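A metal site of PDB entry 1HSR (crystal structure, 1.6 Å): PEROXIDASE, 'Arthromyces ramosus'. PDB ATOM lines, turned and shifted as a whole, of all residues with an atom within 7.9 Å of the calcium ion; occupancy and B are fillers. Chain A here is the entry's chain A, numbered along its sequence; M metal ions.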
ATOM      1  N   PRO A 130      12.130   2.874 -22.001  1.00  0.00           N
ATOM      2  CA  PRO A 130      11.643   2.344 -20.727  1.00  0.00           C
ATOM      3  C   PRO A 130      10.290   1.663 -20.853  1.00  0.00           C
ATOM      4  O   PRO A 130       9.385   2.200 -21.509  1.00  0.00           O
ATOM      5  CB  PRO A 130      11.582   3.552 -19.794  1.00  0.00           C
ATOM      6  CG  PRO A 130      12.642   4.478 -20.364  1.00  0.00           C
ATOM      7  CD  PRO A 130      12.513   4.284 -21.864  1.00  0.00           C
ATOM      8  N   ALA A 182       0.082  -0.973 -30.027  1.00  0.00           N
ATOM      9  CA  ALA A 182       0.752  -0.518 -28.814  1.00  0.00           C
ATOM     10  C   ALA A 182       1.983   0.306 -29.239  1.00  0.00           C
ATOM     11  O   ALA A 182       2.454   1.144 -28.481  1.00  0.00           O
ATOM     12  CB  ALA A 182       1.255  -1.688 -27.950  1.00  0.00           C
ATOM     13  N   ALA A 183       2.520   0.106 -30.456  1.00  0.00           N
ATOM     14  CA  ALA A 183       3.633   0.887 -30.948  1.00  0.00           C
ATOM     15  C   ALA A 183       3.288   2.366 -31.064  1.00  0.00           C
ATOM     16  O   ALA A 183       4.200   3.189 -31.040  1.00  0.00           O
ATOM     17  CB  ALA A 183       4.059   0.393 -32.328  1.00  0.00           C
ATOM     18  N   HIS A 184       2.001   2.779 -31.074  1.00  0.00           N
ATOM     19  CA  HIS A 184       1.659   4.201 -31.092  1.00  0.00           C
ATOM     20  C   HIS A 184       1.853   4.847 -29.719  1.00  0.00           C
ATOM     21  O   HIS A 184       1.668   6.059 -29.523  1.00  0.00           O
ATOM     22  CB  HIS A 184       0.226   4.382 -31.595  1.00  0.00           C
ATOM     23  CG  HIS A 184       0.136   4.343 -33.125  1.00  0.00           C
ATOM     24  ND1 HIS A 184      -0.986   4.790 -33.809  1.00  0.00           N
ATOM     25  CD2 HIS A 184       1.137   3.951 -34.030  1.00  0.00           C
ATOM     26  CE1 HIS A 184      -0.643   4.688 -35.100  1.00  0.00           C
ATOM     27  NE2 HIS A 184       0.564   4.244 -35.269  1.00  0.00           N
ATOM     28  N   SER A 185       2.271   4.051 -28.712  1.00  0.00           N
ATOM     29  CA  SER A 185       2.653   4.553 -27.395  1.00  0.00           C
ATOM     30  C   SER A 185       4.056   5.202 -27.510  1.00  0.00           C
ATOM     31  O   SER A 185       4.482   5.913 -26.589  1.00  0.00           O
ATOM     32  CB  SER A 185       2.746   3.398 -26.395  1.00  0.00           C
ATOM     33  OG  SER A 185       2.923   3.890 -25.076  1.00  0.00           O
ATOM     34  N   LEU A 186       4.808   5.003 -28.595  1.00  0.00           N
ATOM     35  CA  LEU A 186       6.156   5.572 -28.811  1.00  0.00           C
ATOM     36  C   LEU A 186       6.041   6.278 -30.158  1.00  0.00           C
ATOM     37  O   LEU A 186       6.741   5.904 -31.116  1.00  0.00           O
ATOM     38  CB  LEU A 186       7.122   4.392 -28.883  1.00  0.00           C
ATOM     39  CG  LEU A 186       8.083   3.899 -27.792  1.00  0.00           C
ATOM     40  CD1 LEU A 186       7.719   4.383 -26.438  1.00  0.00           C
ATOM     41  CD2 LEU A 186       8.196   2.393 -27.972  1.00  0.00           C
ATOM     42  N   ALA A 187       5.197   7.301 -30.287  1.00  0.00           N
ATOM     43  CA  ALA A 187       4.902   7.843 -31.600  1.00  0.00           C
ATOM     44  C   ALA A 187       4.531   9.306 -31.694  1.00  0.00           C
ATOM     45  O   ALA A 187       3.980   9.904 -30.758  1.00  0.00           O
ATOM     46  CB  ALA A 187       3.757   7.055 -32.207  1.00  0.00           C
ATOM     47  N   LEU A 201       1.397  11.109 -30.081  1.00  0.00           N
ATOM     48  CA  LEU A 201       0.127  10.413 -30.092  1.00  0.00           C
ATOM     49  C   LEU A 201      -0.262  10.075 -28.645  1.00  0.00           C
ATOM     50  O   LEU A 201      -1.404   9.693 -28.398  1.00  0.00           O
ATOM     51  CB  LEU A 201       0.284   9.151 -30.966  1.00  0.00           C
ATOM     52  CG  LEU A 201      -0.154   9.211 -32.461  1.00  0.00           C
ATOM     53  CD1 LEU A 201       0.247  10.517 -33.116  1.00  0.00           C
ATOM     54  CD2 LEU A 201       0.369   7.981 -33.159  1.00  0.00           C
ATOM     55  N   ASP A 202       0.636  10.083 -27.642  1.00  0.00           N
ATOM     56  CA  ASP A 202       0.186   9.960 -26.258  1.00  0.00           C
ATOM     57  C   ASP A 202       1.109  10.880 -25.438  1.00  0.00           C
ATOM     58  O   ASP A 202       2.094  11.416 -25.975  1.00  0.00           O
ATOM     59  CB  ASP A 202       0.239   8.484 -25.719  1.00  0.00           C
ATOM     60  CG  ASP A 202       1.523   7.769 -25.318  1.00  0.00           C
ATOM     61  OD1 ASP A 202       2.626   8.318 -25.405  1.00  0.00           O
ATOM     62  OD2 ASP A 202       1.405   6.609 -24.891  1.00  0.00           O
ATOM     63  N   SER A 203       0.850  11.046 -24.125  1.00  0.00           N
ATOM     64  CA  SER A 203       1.640  11.940 -23.312  1.00  0.00           C
ATOM     65  C   SER A 203       3.020  11.414 -22.926  1.00  0.00           C
ATOM     66  O   SER A 203       3.747  12.157 -22.245  1.00  0.00           O
ATOM     67  CB  SER A 203       0.864  12.271 -22.052  1.00  0.00           C
ATOM     68  OG  SER A 203       0.595  11.101 -21.296  1.00  0.00           O
ATOM     69  N   THR A 204       3.432  10.182 -23.290  1.00  0.00           N
ATOM     70  CA  THR A 204       4.732   9.649 -22.957  1.00  0.00           C
ATOM     71  C   THR A 204       5.347   9.029 -24.186  1.00  0.00           C
ATOM     72  O   THR A 204       5.527   7.805 -24.264  1.00  0.00           O
ATOM     73  CB  THR A 204       4.580   8.637 -21.823  1.00  0.00           C
ATOM     74  OG1 THR A 204       3.631   7.691 -22.293  1.00  0.00           O
ATOM     75  CG2 THR A 204       4.093   9.257 -20.511  1.00  0.00           C
ATOM     76  N   PRO A 205       5.775   9.810 -25.202  1.00  0.00           N
ATOM     77  CA  PRO A 205       6.327   9.260 -26.445  1.00  0.00           C
ATOM     78  C   PRO A 205       7.646   8.511 -26.287  1.00  0.00           C
ATOM     79  O   PRO A 205       8.135   7.895 -27.243  1.00  0.00           O
ATOM     80  CB  PRO A 205       6.406  10.468 -27.380  1.00  0.00           C
ATOM     81  CG  PRO A 205       6.587  11.636 -26.427  1.00  0.00           C
ATOM     82  CD  PRO A 205       5.635  11.265 -25.285  1.00  0.00           C
ATOM     83  N   GLN A 206       8.246   8.633 -25.071  1.00  0.00           N
ATOM     84  CA  GLN A 206       9.468   7.918 -24.766  1.00  0.00           C
ATOM     85  C   GLN A 206       9.219   6.803 -23.778  1.00  0.00           C
ATOM     86  O   GLN A 206      10.212   6.247 -23.295  1.00  0.00           O
ATOM     87  CB  GLN A 206      10.549   8.883 -24.245  1.00  0.00           C
ATOM     88  CG  GLN A 206      11.025   9.780 -25.393  1.00  0.00           C
ATOM     89  CD  GLN A 206      12.216  10.621 -24.948  1.00  0.00           C
ATOM     90  OE1 GLN A 206      12.049  11.524 -24.125  1.00  0.00           O
ATOM     91  NE2 GLN A 206      13.430  10.357 -25.419  1.00  0.00           N
ATOM     92  N   VAL A 207       8.003   6.423 -23.419  1.00  0.00           N
ATOM     93  CA  VAL A 207       7.812   5.324 -22.469  1.00  0.00           C
ATOM     94  C   VAL A 207       6.819   4.357 -23.123  1.00  0.00           C
ATOM     95  O   VAL A 207       5.756   4.805 -23.567  1.00  0.00           O
ATOM     96  CB  VAL A 207       7.214   5.781 -21.113  1.00  0.00           C
ATOM     97  CG1 VAL A 207       7.029   4.562 -20.206  1.00  0.00           C
ATOM     98  CG2 VAL A 207       8.116   6.793 -20.430  1.00  0.00           C
ATOM     99  N   PHE A 208       7.155   3.056 -23.195  1.00  0.00           N
ATOM    100  CA  PHE A 208       6.269   2.078 -23.781  1.00  0.00           C
ATOM    101  C   PHE A 208       5.293   1.697 -22.677  1.00  0.00           C
ATOM    102  O   PHE A 208       5.597   0.914 -21.768  1.00  0.00           O
ATOM    103  CB  PHE A 208       7.077   0.871 -24.225  1.00  0.00           C
ATOM    104  CG  PHE A 208       6.205  -0.155 -24.953  1.00  0.00           C
ATOM    105  CD1 PHE A 208       5.708   0.141 -26.233  1.00  0.00           C
ATOM    106  CD2 PHE A 208       5.916  -1.385 -24.348  1.00  0.00           C
ATOM    107  CE1 PHE A 208       4.915  -0.812 -26.898  1.00  0.00           C
ATOM    108  CE2 PHE A 208       5.135  -2.322 -25.015  1.00  0.00           C
ATOM    109  CZ  PHE A 208       4.636  -2.037 -26.286  1.00  0.00           C
ATOM    110  N   ASP A 209       4.104   2.284 -22.721  1.00  0.00           N
ATOM    111  CA  ASP A 209       3.101   2.117 -21.675  1.00  0.00           C
ATOM    112  C   ASP A 209       1.686   2.138 -22.276  1.00  0.00           C
ATOM    113  O   ASP A 209       1.427   2.353 -23.464  1.00  0.00           O
ATOM    114  CB  ASP A 209       3.252   3.265 -20.628  1.00  0.00           C
ATOM    115  CG  ASP A 209       3.163   4.675 -21.239  1.00  0.00           C
ATOM    116  OD1 ASP A 209       2.761   4.847 -22.410  1.00  0.00           O
ATOM    117  OD2 ASP A 209       3.530   5.622 -20.531  1.00  0.00           O
ATOM    118  N   THR A 210       0.747   2.060 -21.390  1.00  0.00           N
ATOM    119  CA  THR A 210      -0.661   2.026 -21.704  1.00  0.00           C
ATOM    120  C   THR A 210      -1.293   3.412 -22.024  1.00  0.00           C
ATOM    121  O   THR A 210      -2.455   3.473 -22.466  1.00  0.00           O
ATOM    122  CB  THR A 210      -1.039   1.267 -20.423  1.00  0.00           C
ATOM    123  OG1 THR A 210      -1.384  -0.075 -20.749  1.00  0.00           O
ATOM    124  CG2 THR A 210      -1.873   2.138 -19.621  1.00  0.00           C
ATOM    125  N   GLN A 211      -0.591   4.555 -21.828  1.00  0.00           N
ATOM    126  CA  GLN A 211      -1.229   5.857 -22.017  1.00  0.00           C
ATOM    127  C   GLN A 211      -1.911   6.060 -23.356  1.00  0.00           C
ATOM    128  O   GLN A 211      -2.974   6.669 -23.379  1.00  0.00           O
ATOM    129  CB  GLN A 211      -0.199   6.985 -21.795  1.00  0.00           C
ATOM    130  CG  GLN A 211       0.311   7.105 -20.351  1.00  0.00           C
ATOM    131  CD  GLN A 211      -0.818   7.215 -19.324  1.00  0.00           C
ATOM    132  OE1 GLN A 211      -0.835   6.490 -18.326  1.00  0.00           O
ATOM    133  NE2 GLN A 211      -1.797   8.098 -19.496  1.00  0.00           N
ATOM    134  N   PHE A 212      -1.403   5.506 -24.444  1.00  0.00           N
ATOM    135  CA  PHE A 212      -2.005   5.639 -25.766  1.00  0.00           C
ATOM    136  C   PHE A 212      -3.438   5.114 -25.774  1.00  0.00           C
ATOM    137  O   PHE A 212      -4.307   5.809 -26.316  1.00  0.00           O
ATOM    138  CB  PHE A 212      -1.150   4.908 -26.795  1.00  0.00           C
ATOM    139  CG  PHE A 212      -1.844   4.734 -28.130  1.00  0.00           C
ATOM    140  CD1 PHE A 212      -2.094   5.832 -28.967  1.00  0.00           C
ATOM    141  CD2 PHE A 212      -2.266   3.445 -28.491  1.00  0.00           C
ATOM    142  CE1 PHE A 212      -2.783   5.641 -30.168  1.00  0.00           C
ATOM    143  CE2 PHE A 212      -2.949   3.262 -29.693  1.00  0.00           C
ATOM    144  CZ  PHE A 212      -3.205   4.352 -30.529  1.00  0.00           C
ATOM    145  N   TYR A 213      -3.710   3.958 -25.166  1.00  0.00           N
ATOM    146  CA  TYR A 213      -5.055   3.380 -25.180  1.00  0.00           C
ATOM    147  C   TYR A 213      -5.997   4.211 -24.320  1.00  0.00           C
ATOM    148  O   TYR A 213      -7.163   4.405 -24.694  1.00  0.00           O
ATOM    149  CB  TYR A 213      -4.969   1.953 -24.667  1.00  0.00           C
ATOM    150  CG  TYR A 213      -4.226   1.034 -25.647  1.00  0.00           C
ATOM    151  CD1 TYR A 213      -4.825   0.578 -26.828  1.00  0.00           C
ATOM    152  CD2 TYR A 213      -2.918   0.606 -25.332  1.00  0.00           C
ATOM    153  CE1 TYR A 213      -4.142  -0.309 -27.670  1.00  0.00           C
ATOM    154  CE2 TYR A 213      -2.239  -0.279 -26.183  1.00  0.00           C
ATOM    155  CZ  TYR A 213      -2.860  -0.740 -27.330  1.00  0.00           C
ATOM    156  OH  TYR A 213      -2.200  -1.665 -28.088  1.00  0.00           O
ATOM    157  N   GLU A 215      -5.704   7.587 -23.534  1.00  0.00           N
ATOM    158  CA  GLU A 215      -5.908   8.913 -24.073  1.00  0.00           C
ATOM    159  C   GLU A 215      -6.651   8.977 -25.387  1.00  0.00           C
ATOM    160  O   GLU A 215      -7.303   9.988 -25.603  1.00  0.00           O
ATOM    161  CB  GLU A 215      -4.540   9.613 -24.188  1.00  0.00           C
ATOM    162  CG  GLU A 215      -3.927   9.778 -22.775  1.00  0.00           C
ATOM    163  CD  GLU A 215      -2.466  10.225 -22.713  1.00  0.00           C
ATOM    164  OE1 GLU A 215      -1.934  10.747 -23.681  1.00  0.00           O
ATOM    165  OE2 GLU A 215      -1.840  10.024 -21.688  1.00  0.00           O
ATOM    166  N   ASN A 266       0.379  -2.462 -17.970  1.00  0.00           N
ATOM    167  CA  ASN A 266       1.499  -2.420 -18.896  1.00  0.00           C
ATOM    168  C   ASN A 266       2.046  -3.816 -19.138  1.00  0.00           C
ATOM    169  O   ASN A 266       2.612  -4.112 -20.187  1.00  0.00           O
ATOM    170  CB  ASN A 266       2.617  -1.578 -18.339  1.00  0.00           C
ATOM    171  CG  ASN A 266       2.290  -0.103 -18.335  1.00  0.00           C
ATOM    172  OD1 ASN A 266       1.883   0.448 -19.345  1.00  0.00           O
ATOM    173  ND2 ASN A 266       2.420   0.593 -17.220  1.00  0.00           N
ATOM    174  N   MET A 269      -0.184  -5.615 -21.704  1.00  0.00           N
ATOM    175  CA  MET A 269       0.047  -4.984 -22.981  1.00  0.00           C
ATOM    176  C   MET A 269       1.384  -5.452 -23.621  1.00  0.00           C
ATOM    177  O   MET A 269       1.419  -5.852 -24.791  1.00  0.00           O
ATOM    178  CB  MET A 269       0.058  -3.446 -22.811  1.00  0.00           C
ATOM    179  CG  MET A 269       0.429  -2.735 -24.128  1.00  0.00           C
ATOM    180  SD  MET A 269       0.669  -0.964 -23.926  1.00  0.00           S
ATOM    181  CE  MET A 269       2.315  -1.052 -23.273  1.00  0.00           C
ATOM    182  N   ASN A 303       9.601   0.387 -16.338  1.00  0.00           N
ATOM    183  CA  ASN A 303       8.797   1.580 -16.173  1.00  0.00           C
ATOM    184  C   ASN A 303       8.032   1.371 -14.869  1.00  0.00           C
ATOM    185  O   ASN A 303       7.243   0.432 -14.737  1.00  0.00           O
ATOM    186  CB  ASN A 303       7.814   1.723 -17.318  1.00  0.00           C
ATOM    187  CG  ASN A 303       6.698   2.722 -17.008  1.00  0.00           C
ATOM    188  OD1 ASN A 303       6.921   3.680 -16.264  1.00  0.00           O
ATOM    189  ND2 ASN A 303       5.479   2.534 -17.499  1.00  0.00           N
HETATM  190 CA    CA M   1       3.704   6.126 -24.240  1.00  0.00          CA
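The side-chain carboxylate (OD1) of Asp 209 sits close to the backbone NH (N) of Gln 211 (3.4 Å).
The side-chain carboxylate (OD2) of Asp 202 sits close to the backbone NH (N) of Phe 212 (3.0 Å).
The calcium ion is bound by the side-chain carboxylate (OD1) of Asp 209, the side-chain carboxylate (OD2) of Asp 202, the backbone carbonyl oxygen (O) of Thr 204, the backbone carbonyl oxygen (O) of Ser 185, the side-chain hydroxyl (OG1) of Thr 204, the side-chain hydroxyl (OG) of Ser 185, the backbone carbonyl oxygen (O) of Val 207 and the side-chain carboxylate (OD1) of Asp 202.
The calcium ion has eight donor atoms within binding distance.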
